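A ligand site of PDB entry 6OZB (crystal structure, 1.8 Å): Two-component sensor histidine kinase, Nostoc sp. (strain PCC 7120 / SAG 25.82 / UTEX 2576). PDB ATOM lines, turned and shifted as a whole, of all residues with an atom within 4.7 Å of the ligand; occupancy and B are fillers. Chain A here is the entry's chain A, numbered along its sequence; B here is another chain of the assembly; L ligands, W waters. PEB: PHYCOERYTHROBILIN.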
ATOM      1  N   MET A  53       6.403  11.155  32.026  1.00  0.00           N
ATOM      2  CA  MET A  53       6.761  11.358  30.619  1.00  0.00           C
ATOM      3  C   MET A  53       5.630  12.029  29.870  1.00  0.00           C
ATOM      4  O   MET A  53       4.443  11.845  30.197  1.00  0.00           O
ATOM      5  CB  MET A  53       7.096  10.027  29.936  1.00  0.00           C
ATOM      6  CG  MET A  53       8.253   9.214  30.563  1.00  0.00           C
ATOM      7  SD  MET A  53       8.442   7.578  29.861  1.00  0.00           S
ATOM      8  CE  MET A  53       6.922   6.820  30.367  1.00  0.00           C
ATOM      9  N   TYR A  55       4.291  11.890  26.046  1.00  0.00           N
ATOM     10  CA  TYR A  55       4.354  11.025  24.865  1.00  0.00           C
ATOM     11  C   TYR A  55       3.621  11.728  23.730  1.00  0.00           C
ATOM     12  O   TYR A  55       2.478  12.097  23.917  1.00  0.00           O
ATOM     13  CB  TYR A  55       3.703   9.681  25.184  1.00  0.00           C
ATOM     14  CG  TYR A  55       3.773   8.614  24.109  1.00  0.00           C
ATOM     15  CD1 TYR A  55       4.950   7.908  23.863  1.00  0.00           C
ATOM     16  CD2 TYR A  55       2.655   8.294  23.372  1.00  0.00           C
ATOM     17  CE1 TYR A  55       4.999   6.920  22.893  1.00  0.00           C
ATOM     18  CE2 TYR A  55       2.684   7.287  22.415  1.00  0.00           C
ATOM     19  CZ  TYR A  55       3.874   6.600  22.187  1.00  0.00           C
ATOM     20  OH  TYR A  55       3.922   5.630  21.233  1.00  0.00           O
ATOM     21  N   LEU A  78      13.474   6.604  29.127  1.00  0.00           N
ATOM     22  CA  LEU A  78      12.901   6.272  27.823  1.00  0.00           C
ATOM     23  C   LEU A  78      12.879   7.491  26.870  1.00  0.00           C
ATOM     24  O   LEU A  78      12.327   7.414  25.787  1.00  0.00           O
ATOM     25  CB  LEU A  78      11.495   5.720  27.970  1.00  0.00           C
ATOM     26  CG  LEU A  78      11.331   4.531  28.922  1.00  0.00           C
ATOM     27  CD1 LEU A  78       9.922   4.035  28.933  1.00  0.00           C
ATOM     28  CD2 LEU A  78      12.292   3.421  28.534  1.00  0.00           C
ATOM     29  N   PHE A  83       7.720   4.320  20.121  1.00  0.00           N
ATOM     30  CA  PHE A  83       6.926   3.098  20.348  1.00  0.00           C
ATOM     31  C   PHE A  83       5.885   2.933  19.231  1.00  0.00           C
ATOM     32  O   PHE A  83       5.332   3.901  18.739  1.00  0.00           O
ATOM     33  CB  PHE A  83       6.271   3.165  21.730  1.00  0.00           C
ATOM     34  CG  PHE A  83       7.241   3.152  22.853  1.00  0.00           C
ATOM     35  CD1 PHE A  83       7.900   4.313  23.219  1.00  0.00           C
ATOM     36  CD2 PHE A  83       7.553   1.981  23.496  1.00  0.00           C
ATOM     37  CE1 PHE A  83       8.827   4.319  24.245  1.00  0.00           C
ATOM     38  CE2 PHE A  83       8.474   1.968  24.536  1.00  0.00           C
ATOM     39  CZ  PHE A  83       9.110   3.151  24.908  1.00  0.00           C
ATOM     40  N   ASP A  86       0.742  -0.270  17.528  1.00  0.00           N
ATOM     41  CA  ASP A  86       0.084  -1.457  18.068  1.00  0.00           C
ATOM     42  C   ASP A  86       0.209  -1.589  19.595  1.00  0.00           C
ATOM     43  O   ASP A  86      -0.455  -2.434  20.203  1.00  0.00           O
ATOM     44  CB  ASP A  86       0.632  -2.695  17.370  1.00  0.00           C
ATOM     45  CG  ASP A  86       0.136  -2.811  15.928  1.00  0.00           C
ATOM     46  OD1 ASP A  86      -0.758  -2.022  15.528  1.00  0.00           O
ATOM     47  OD2 ASP A  86       0.636  -3.691  15.192  1.00  0.00           O
ATOM     48  N   ASP A  87       1.055  -0.769  20.225  1.00  0.00           N
ATOM     49  CA  ASP A  87       1.201  -0.798  21.689  1.00  0.00           C
ATOM     50  C   ASP A  87      -0.100  -0.374  22.342  1.00  0.00           C
ATOM     51  O   ASP A  87      -0.387  -0.731  23.488  1.00  0.00           O
ATOM     52  CB  ASP A  87       2.348   0.093  22.179  1.00  0.00           C
ATOM     53  CG  ASP A  87       3.719  -0.559  21.978  1.00  0.00           C
ATOM     54  OD1 ASP A  87       3.801  -1.540  21.191  1.00  0.00           O
ATOM     55  OD2 ASP A  87       4.691  -0.079  22.604  1.00  0.00           O
ATOM     56  N   ILE A  88      -0.870   0.410  21.587  1.00  0.00           N
ATOM     57  CA  ILE A  88      -2.187   0.885  22.013  1.00  0.00           C
ATOM     58  C   ILE A  88      -3.207   0.423  20.993  1.00  0.00           C
ATOM     59  O   ILE A  88      -3.338   1.054  19.919  1.00  0.00           O
ATOM     60  CB  ILE A  88      -2.248   2.399  22.120  1.00  0.00           C
ATOM     61  CG1 ILE A  88      -1.128   2.945  22.992  1.00  0.00           C
ATOM     62  CG2 ILE A  88      -3.612   2.831  22.667  1.00  0.00           C
ATOM     63  CD1 ILE A  88      -1.067   4.444  23.085  1.00  0.00           C
ATOM     64  N   PRO A  89      -3.925  -0.679  21.277  1.00  0.00           N
ATOM     65  CA  PRO A  89      -4.895  -1.240  20.320  1.00  0.00           C
ATOM     66  C   PRO A  89      -6.097  -0.351  20.085  1.00  0.00           C
ATOM     67  O   PRO A  89      -6.317   0.587  20.857  1.00  0.00           O
ATOM     68  CB  PRO A  89      -5.339  -2.549  20.985  1.00  0.00           C
ATOM     69  CG  PRO A  89      -4.258  -2.871  21.922  1.00  0.00           C
ATOM     70  CD  PRO A  89      -3.812  -1.542  22.462  1.00  0.00           C
ATOM     71  N   ALA A  92      -8.564   0.505  23.060  1.00  0.00           N
ATOM     72  CA  ALA A  92      -7.942   1.437  24.009  1.00  0.00           C
ATOM     73  C   ALA A  92      -7.868   2.843  23.416  1.00  0.00           C
ATOM     74  O   ALA A  92      -8.148   3.827  24.085  1.00  0.00           O
ATOM     75  CB  ALA A  92      -6.560   0.953  24.375  1.00  0.00           C
ATOM     76  N   SER A 103      -6.678   6.309  32.887  1.00  0.00           N
ATOM     77  CA  SER A 103      -6.473   4.902  33.220  1.00  0.00           C
ATOM     78  C   SER A 103      -5.416   4.694  34.286  1.00  0.00           C
ATOM     79  O   SER A 103      -4.309   5.239  34.205  1.00  0.00           O
ATOM     80  CB  SER A 103      -6.059   4.094  31.984  1.00  0.00           C
ATOM     81  OG  SER A 103      -7.092   4.072  31.021  1.00  0.00           O
ATOM     82  N   VAL A 105      -3.457   1.535  36.082  1.00  0.00           N
ATOM     83  CA  VAL A 105      -3.134   0.103  36.127  1.00  0.00           C
ATOM     84  C   VAL A 105      -2.438  -0.240  37.428  1.00  0.00           C
ATOM     85  O   VAL A 105      -1.458   0.430  37.829  1.00  0.00           O
ATOM     86  CB  VAL A 105      -2.252  -0.355  34.939  1.00  0.00           C
ATOM     87  CG1 VAL A 105      -2.003  -1.841  34.994  1.00  0.00           C
ATOM     88  CG2 VAL A 105      -2.918  -0.027  33.622  1.00  0.00           C
ATOM     89  N   ILE A 112      -7.309  -2.681  36.026  1.00  0.00           N
ATOM     90  CA  ILE A 112      -7.201  -1.352  35.462  1.00  0.00           C
ATOM     91  C   ILE A 112      -8.454  -0.591  35.785  1.00  0.00           C
ATOM     92  O   ILE A 112      -9.555  -1.104  35.644  1.00  0.00           O
ATOM     93  CB  ILE A 112      -6.964  -1.405  33.923  1.00  0.00           C
ATOM     94  CG1 ILE A 112      -6.863   0.021  33.347  1.00  0.00           C
ATOM     95  CG2 ILE A 112      -8.031  -2.201  33.250  1.00  0.00           C
ATOM     96  CD1 ILE A 112      -6.369   0.118  31.874  1.00  0.00           C
ATOM     97  N   GLN A 114     -10.729   2.867  35.124  1.00  0.00           N
ATOM     98  CA  GLN A 114     -10.909   3.843  34.077  1.00  0.00           C
ATOM     99  C   GLN A 114     -11.967   4.825  34.480  1.00  0.00           C
ATOM    100  O   GLN A 114     -13.002   4.474  35.053  1.00  0.00           O
ATOM    101  CB  GLN A 114     -11.212   3.137  32.759  1.00  0.00           C
ATOM    102  CG  GLN A 114      -9.915   2.474  32.241  1.00  0.00           C
ATOM    103  CD  GLN A 114     -10.036   1.891  30.860  1.00  0.00           C
ATOM    104  OE1 GLN A 114     -11.003   1.225  30.541  1.00  0.00           O
ATOM    105  NE2 GLN A 114      -9.002   2.101  30.042  1.00  0.00           N
ATOM    106  N   ARG A 133     -11.544  -3.172  36.364  1.00  0.00           N
ATOM    107  CA  ARG A 133     -11.765  -4.447  35.664  1.00  0.00           C
ATOM    108  C   ARG A 133     -10.421  -5.122  35.437  1.00  0.00           C
ATOM    109  O   ARG A 133      -9.377  -4.512  35.606  1.00  0.00           O
ATOM    110  CB  ARG A 133     -12.466  -4.228  34.329  1.00  0.00           C
ATOM    111  CG  ARG A 133     -11.631  -3.360  33.372  1.00  0.00           C
ATOM    112  CD  ARG A 133     -12.209  -3.340  31.980  1.00  0.00           C
ATOM    113  NE  ARG A 133     -11.532  -2.373  31.100  1.00  0.00           N
ATOM    114  CZ  ARG A 133     -10.380  -2.608  30.464  1.00  0.00           C
ATOM    115  NH1 ARG A 133      -9.760  -3.770  30.611  1.00  0.00           N
ATOM    116  NH2 ARG A 133      -9.843  -1.675  29.669  1.00  0.00           N
ATOM    117  N   PRO A 134     -10.425  -6.403  35.062  1.00  0.00           N
ATOM    118  CA  PRO A 134      -9.139  -7.047  34.795  1.00  0.00           C
ATOM    119  C   PRO A 134      -8.445  -6.440  33.594  1.00  0.00           C
ATOM    120  O   PRO A 134      -9.111  -6.145  32.591  1.00  0.00           O
ATOM    121  CB  PRO A 134      -9.514  -8.502  34.551  1.00  0.00           C
ATOM    122  CG  PRO A 134     -10.842  -8.655  35.298  1.00  0.00           C
ATOM    123  CD  PRO A 134     -11.535  -7.365  35.060  1.00  0.00           C
ATOM    124  N   VAL A 135      -7.136  -6.223  33.703  1.00  0.00           N
ATOM    125  CA  VAL A 135      -6.380  -5.605  32.625  1.00  0.00           C
ATOM    126  C   VAL A 135      -5.805  -6.705  31.723  1.00  0.00           C
ATOM    127  O   VAL A 135      -5.450  -7.775  32.181  1.00  0.00           O
ATOM    128  CB  VAL A 135      -5.259  -4.668  33.165  1.00  0.00           C
ATOM    129  CG1 VAL A 135      -4.190  -5.455  33.876  1.00  0.00           C
ATOM    130  CG2 VAL A 135      -4.656  -3.808  32.019  1.00  0.00           C
ATOM    131  N   ASP A 136      -5.750  -6.456  30.431  1.00  0.00           N
ATOM    132  CA  ASP A 136      -5.204  -7.454  29.506  1.00  0.00           C
ATOM    133  C   ASP A 136      -3.780  -7.847  29.905  1.00  0.00           C
ATOM    134  O   ASP A 136      -2.949  -6.985  30.270  1.00  0.00           O
ATOM    135  CB  ASP A 136      -5.226  -6.922  28.078  1.00  0.00           C
ATOM    136  CG  ASP A 136      -5.061  -8.021  27.053  1.00  0.00           C
ATOM    137  OD1 ASP A 136      -3.937  -8.503  26.890  1.00  0.00           O
ATOM    138  OD2 ASP A 136      -6.060  -8.425  26.420  1.00  0.00           O
ATOM    139  N   CYS A 138      -1.331  -8.780  28.164  1.00  0.00           N
ATOM    140  CA  CYS A 138      -0.274  -8.233  27.324  1.00  0.00           C
ATOM    141  C   CYS A 138       0.236  -6.902  27.885  1.00  0.00           C
ATOM    142  O   CYS A 138       1.440  -6.604  27.871  1.00  0.00           O
ATOM    143  CB  CYS A 138      -0.730  -8.044  25.899  1.00  0.00           C
ATOM    144  SG  CYS A 138       0.589  -7.462  24.832  1.00  0.00           S
ATOM    145  N   HIS A 139      -0.704  -6.077  28.356  1.00  0.00           N
ATOM    146  CA  HIS A 139      -0.377  -4.766  28.887  1.00  0.00           C
ATOM    147  C   HIS A 139       0.295  -4.904  30.235  1.00  0.00           C
ATOM    148  O   HIS A 139       1.205  -4.135  30.550  1.00  0.00           O
ATOM    149  CB  HIS A 139      -1.629  -3.914  28.996  1.00  0.00           C
ATOM    150  CG  HIS A 139      -1.388  -2.476  29.312  1.00  0.00           C
ATOM    151  ND1 HIS A 139      -0.362  -1.739  28.747  1.00  0.00           N
ATOM    152  CD2 HIS A 139      -2.084  -1.628  30.102  1.00  0.00           C
ATOM    153  CE1 HIS A 139      -0.440  -0.491  29.199  1.00  0.00           C
ATOM    154  NE2 HIS A 139      -1.469  -0.394  30.022  1.00  0.00           N
ATOM    155  N   TYR A 142       3.803  -5.794  29.484  1.00  0.00           N
ATOM    156  CA  TYR A 142       4.467  -4.600  28.943  1.00  0.00           C
ATOM    157  C   TYR A 142       5.006  -3.711  30.053  1.00  0.00           C
ATOM    158  O   TYR A 142       6.142  -3.252  30.002  1.00  0.00           O
ATOM    159  CB  TYR A 142       3.451  -3.830  28.104  1.00  0.00           C
ATOM    160  CG  TYR A 142       3.893  -2.582  27.391  1.00  0.00           C
ATOM    161  CD1 TYR A 142       4.441  -2.654  26.121  1.00  0.00           C
ATOM    162  CD2 TYR A 142       3.642  -1.323  27.949  1.00  0.00           C
ATOM    163  CE1 TYR A 142       4.785  -1.518  25.430  1.00  0.00           C
ATOM    164  CE2 TYR A 142       3.990  -0.154  27.241  1.00  0.00           C
ATOM    165  CZ  TYR A 142       4.557  -0.282  25.973  1.00  0.00           C
ATOM    166  OH  TYR A 142       4.897   0.823  25.238  1.00  0.00           O
ATOM    167  N   LEU A 143       4.155  -3.442  31.037  1.00  0.00           N
ATOM    168  CA  LEU A 143       4.520  -2.600  32.162  1.00  0.00           C
ATOM    169  C   LEU A 143       5.571  -3.280  33.065  1.00  0.00           C
ATOM    170  O   LEU A 143       6.524  -2.623  33.478  1.00  0.00           O
ATOM    171  CB  LEU A 143       3.279  -2.238  32.973  1.00  0.00           C
ATOM    172  CG  LEU A 143       2.265  -1.339  32.259  1.00  0.00           C
ATOM    173  CD1 LEU A 143       1.055  -1.183  33.116  1.00  0.00           C
ATOM    174  CD2 LEU A 143       2.830   0.016  31.957  1.00  0.00           C
ATOM    175  N   MET A 146       9.005  -3.073  31.878  1.00  0.00           N
ATOM    176  CA  MET A 146       9.604  -1.755  32.086  1.00  0.00           C
ATOM    177  C   MET A 146       9.978  -1.527  33.551  1.00  0.00           C
ATOM    178  O   MET A 146      10.571  -0.515  33.888  1.00  0.00           O
ATOM    179  CB  MET A 146       8.630  -0.663  31.639  1.00  0.00           C
ATOM    180  CG  MET A 146       8.553  -0.502  30.127  1.00  0.00           C
ATOM    181  SD  MET A 146       7.508   0.941  29.784  1.00  0.00           S
ATOM    182  CE  MET A 146       7.814   1.207  28.055  1.00  0.00           C
ATOM    183  N   SER A 151       0.791   2.458  36.838  1.00  0.00           N
ATOM    184  CA  SER A 151       0.737   3.374  35.715  1.00  0.00           C
ATOM    185  C   SER A 151      -0.533   4.205  35.767  1.00  0.00           C
ATOM    186  O   SER A 151      -1.616   3.692  36.046  1.00  0.00           O
ATOM    187  CB  SER A 151       0.780   2.594  34.402  1.00  0.00           C
ATOM    188  OG  SER A 151       0.627   3.423  33.274  1.00  0.00           O
ATOM    189  N   VAL A 153      -2.373   7.194  33.223  1.00  0.00           N
ATOM    190  CA  VAL A 153      -2.279   7.865  31.921  1.00  0.00           C
ATOM    191  C   VAL A 153      -3.481   8.767  31.683  1.00  0.00           C
ATOM    192  O   VAL A 153      -4.630   8.371  31.925  1.00  0.00           O
ATOM    193  CB  VAL A 153      -2.197   6.843  30.785  1.00  0.00           C
ATOM    194  CG1 VAL A 153      -2.280   7.518  29.396  1.00  0.00           C
ATOM    195  CG2 VAL A 153      -0.910   6.047  30.920  1.00  0.00           C
ATOM    196  N   LEU A 165       0.086  11.870  25.350  1.00  0.00           N
ATOM    197  CA  LEU A 165      -0.267  11.331  26.647  1.00  0.00           C
ATOM    198  C   LEU A 165       0.636  11.919  27.719  1.00  0.00           C
ATOM    199  O   LEU A 165       1.830  12.102  27.484  1.00  0.00           O
ATOM    200  CB  LEU A 165      -0.100   9.806  26.688  1.00  0.00           C
ATOM    201  CG  LEU A 165      -0.762   8.952  25.609  1.00  0.00           C
ATOM    202  CD1 LEU A 165      -0.284   7.514  25.772  1.00  0.00           C
ATOM    203  CD2 LEU A 165      -2.269   8.992  25.643  1.00  0.00           C
ATOM    204  N   VAL A 167       2.049  10.515  31.072  1.00  0.00           N
ATOM    205  CA  VAL A 167       2.264   9.136  31.595  1.00  0.00           C
ATOM    206  C   VAL A 167       2.999   9.208  32.919  1.00  0.00           C
ATOM    207  O   VAL A 167       4.073   9.803  33.010  1.00  0.00           O
ATOM    208  CB  VAL A 167       3.035   8.265  30.607  1.00  0.00           C
ATOM    209  CG1 VAL A 167       3.163   6.826  31.120  1.00  0.00           C
ATOM    210  CG2 VAL A 167       2.349   8.301  29.230  1.00  0.00           C
ATOM    211  N   HIS A 169       4.488   6.775  35.895  1.00  0.00           N
ATOM    212  CA  HIS A 169       4.894   5.423  36.243  1.00  0.00           C
ATOM    213  C   HIS A 169       5.569   5.349  37.587  1.00  0.00           C
ATOM    214  O   HIS A 169       6.386   6.218  37.919  1.00  0.00           O
ATOM    215  CB  HIS A 169       5.873   4.888  35.228  1.00  0.00           C
ATOM    216  CG  HIS A 169       5.276   4.495  33.916  1.00  0.00           C
ATOM    217  ND1 HIS A 169       6.052   4.217  32.819  1.00  0.00           N
ATOM    218  CD2 HIS A 169       3.992   4.273  33.543  1.00  0.00           C
ATOM    219  CE1 HIS A 169       5.272   3.870  31.810  1.00  0.00           C
ATOM    220  NE2 HIS A 169       4.018   3.896  32.223  1.00  0.00           N
ATOM    221  N   THR B 175      -9.572 -11.023  28.445  1.00  0.00           N
ATOM    222  CA  THR B 175     -10.475  -9.931  28.798  1.00  0.00           C
ATOM    223  C   THR B 175     -11.747 -10.087  28.001  1.00  0.00           C
ATOM    224  O   THR B 175     -11.727 -10.580  26.880  1.00  0.00           O
ATOM    225  CB  THR B 175      -9.869  -8.557  28.502  1.00  0.00           C
ATOM    226  OG1 THR B 175      -9.580  -8.477  27.120  1.00  0.00           O
ATOM    227  CG2 THR B 175      -8.610  -8.334  29.315  1.00  0.00           C
HETATM  228  CHC PEB L   1       1.047   2.105  25.914  1.00  0.00           C
HETATM  229  NC  PEB L   1      -0.947   0.526  26.148  1.00  0.00           N
HETATM  230  C1C PEB L   1      -2.244   0.560  26.547  1.00  0.00           C
HETATM  231  C2C PEB L   1      -2.565   1.827  26.969  1.00  0.00           C
HETATM  232  C3C PEB L   1      -1.440   2.613  26.825  1.00  0.00           C
HETATM  233  C4C PEB L   1      -0.428   1.787  26.325  1.00  0.00           C
HETATM  234  CMC PEB L   1      -1.365   4.094  27.158  1.00  0.00           C
HETATM  235  CAC PEB L   1      -3.983   2.220  27.491  1.00  0.00           C
HETATM  236  CBC PEB L   1      -4.216   1.780  28.933  1.00  0.00           C
HETATM  237  CGC PEB L   1      -3.394   2.591  29.893  1.00  0.00           C
HETATM  238  O1C PEB L   1      -3.561   3.840  29.882  1.00  0.00           O
HETATM  239  O2C PEB L   1      -2.591   2.032  30.701  1.00  0.00           O
HETATM  240  ND  PEB L   1       1.738   3.215  27.942  1.00  0.00           N
HETATM  241  C1D PEB L   1       1.578   3.342  26.435  1.00  0.00           C
HETATM  242  C2D PEB L   1       2.953   3.508  25.963  1.00  0.00           C
HETATM  243  C3D PEB L   1       3.818   3.670  27.025  1.00  0.00           C
HETATM  244  C4D PEB L   1       3.165   3.438  28.267  1.00  0.00           C
HETATM  245  CMD PEB L   1       3.344   3.662  24.454  1.00  0.00           C
HETATM  246  CAD PEB L   1       5.341   3.809  26.808  1.00  0.00           C
HETATM  247  CBD PEB L   1       6.094   4.412  27.770  1.00  0.00           C
HETATM  248  OD  PEB L   1       3.618   3.424  29.398  1.00  0.00           O
HETATM  249  NA  PEB L   1       0.525  -3.797  24.090  1.00  0.00           N
HETATM  250  C1A PEB L   1       1.786  -4.177  23.550  1.00  0.00           C
HETATM  251  C2A PEB L   1       1.631  -5.384  22.673  1.00  0.00           C
HETATM  252  C3A PEB L   1       0.164  -5.760  22.688  1.00  0.00           C
HETATM  253  C4A PEB L   1      -0.493  -4.706  23.608  1.00  0.00           C
HETATM  254  CMA PEB L   1       2.117  -5.088  21.218  1.00  0.00           C
HETATM  255  CBA PEB L   1       0.345  -8.233  22.148  1.00  0.00           C
HETATM  256  OA  PEB L   1       2.815  -3.571  23.771  1.00  0.00           O
HETATM  257  CHA PEB L   1      -1.781  -4.779  23.980  1.00  0.00           C
HETATM  258  CAA PEB L   1      -0.206  -7.176  23.142  1.00  0.00           C
HETATM  259  NB  PEB L   1      -1.996  -2.407  25.227  1.00  0.00           N
HETATM  260  C1B PEB L   1      -2.472  -3.736  24.830  1.00  0.00           C
HETATM  261  C2B PEB L   1      -3.825  -3.990  25.291  1.00  0.00           C
HETATM  262  C3B PEB L   1      -4.218  -2.839  26.033  1.00  0.00           C
HETATM  263  C4B PEB L   1      -3.119  -1.819  26.001  1.00  0.00           C
HETATM  264  CHB PEB L   1      -3.262  -0.592  26.610  1.00  0.00           C
HETATM  265  CMB PEB L   1      -4.633  -5.259  25.077  1.00  0.00           C
HETATM  266  CAB PEB L   1      -5.549  -2.674  26.741  1.00  0.00           C
HETATM  267  CBB PEB L   1      -5.292  -3.044  28.201  1.00  0.00           C
HETATM  268  CGB PEB L   1      -6.622  -2.985  28.922  1.00  0.00           C
HETATM  269  O1B PEB L   1      -7.055  -4.048  29.451  1.00  0.00           O
HETATM  270  O2B PEB L   1      -7.252  -1.890  28.932  1.00  0.00           O
HETATM  271  O   HOH W   1       5.157  -4.392  22.741  1.00  0.00           O
HETATM  272  O   HOH W   2      -5.815   4.867  28.791  1.00  0.00           O
HETATM  273  O   HOH W   3      -2.085   3.495  32.882  1.00  0.00           O
HETATM  274  O   HOH W   4       0.871  -1.900  26.182  1.00  0.00           O
HETATM  275  O   HOH W   5       0.208   2.642  30.373  1.00  0.00           O
HETATM  276  O   HOH W   6      -8.813  -4.626  27.136  1.00  0.00           O
HETATM  277  O   HOH W   7      -7.944   0.398  27.759  1.00  0.00           O
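The guanidinium group of Arg 133 is in salt-bridge range of an oxygen (O2B) of the ligand, 2.7 Å away.
A ring nitrogen (NE2) of His 139 lies within hydrogen-bond range of an oxygen (O2C) of the ligand (2.8 Å).
The side-chain sulfur of Cys 138 is covalently linked to a carbon (CAA) of the ligand.
The backbone NH of Asp 136 lies within hydrogen-bond range of an oxygen (O1B) of the ligand, 2.9 Å away.
OD of the ligand is in hydrogen-bond range of NE2 of His 169 (2.9 Å).
A nitrogen (NC) of the ligand is in hydrogen-bond range of the backbone carbonyl oxygen (O) of Asp 87, at 3.0 Å.
The backbone NH (N) of Met 53 is in hydrogen-bond range of the backbone carbonyl oxygen (O) of Val 167, 2.9 Å away.
The side-chain carboxylate of Asp 87 is in hydrogen-bond range of the side-chain hydroxyl of Tyr 142 (2.8 Å).
OH of Tyr 55 sits at hydrogen-bond distance from O of Phe 83, 3.3 Å away.
O of Tyr 55 is in hydrogen-bond range of N of Leu 165 (2.8 Å).
The side-chain amide oxygen (OE1) of Gln 114 is in hydrogen-bond range of the guanidinium group (NH2) of Arg 133.
The backbone carbonyl oxygen (O) of Ser 103 sits at hydrogen-bond distance from the backbone NH (N) of Val 153 (2.9 Å).
The backbone NH (N) of Val 105 sits at hydrogen-bond distance from the backbone carbonyl oxygen (O) of Ser 151, at 2.8 Å.
The backbone NH (N) of Ile 112 is in hydrogen-bond range of the backbone carbonyl oxygen (O) of Arg 133.
Residues that only touch the ligand: Tyr 142 (3.0 Å), Ser 103 (3.3 Å), Pro 89 (3.4 Å), Val 153 (3.4 Å), Val 135 (3.5 Å), Val 105 (3.6 Å), Ile 88 (3.6 Å), Met 53 (3.6 Å), Met 146 (3.6 Å), Ile 112 (3.7 Å), Tyr 55 (3.7 Å), Asp 86 (3.8 Å), Val 167 (3.8 Å) and Leu 165 (3.8 Å).
Hydrophobic or aromatic side chains that line the ligand: Met 53, Tyr 55, Ile 88, Pro 89, Val 105, Ile 112, Val 135, His 139, Tyr 142, Met 146, Val 153, Leu 165, Val 167 and His 169.
20 residues have an atom within 4 Å of the ligand: Met 53, Tyr 55, Asp 86, Asp 87, Ile 88, Pro 89, Ser 103, Val 105, Ile 112, Arg 133, Val 135, Asp 136, Cys 138, His 139, Tyr 142, Met 146, Val 153, Leu 165, Val 167 and His 169.
The nearest printed residue that does not touch the ligand is Leu 78 (4.02 Å).
Water W7 lies within hydrogen-bond range of an oxygen (O2B) of the ligand (2.7 Å), the side-chain amide nitrogen (NE2) of Gln 114 (3.0 Å) and the guanidinium group (NH2) of Arg 133 (3.4 Å).
Water W3 lies within hydrogen-bond range of O2C of the ligand, OG of Ser 151 and O of Ser 103.
Water W2 lies within hydrogen-bond range of OG of Ser 103 (2.7 Å) and O1C of the ligand (2.7 Å).
Water W4 lies within hydrogen-bond range of NA of the ligand (2.8 Å), ND1 of His 139 (2.9 Å) and O of Asp 87 (3.2 Å).
Water W5 lies within hydrogen-bond range of O2C of the ligand (2.9 Å), OG of Ser 151 (3.0 Å) and NE2 of His 139 (3.5 Å).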
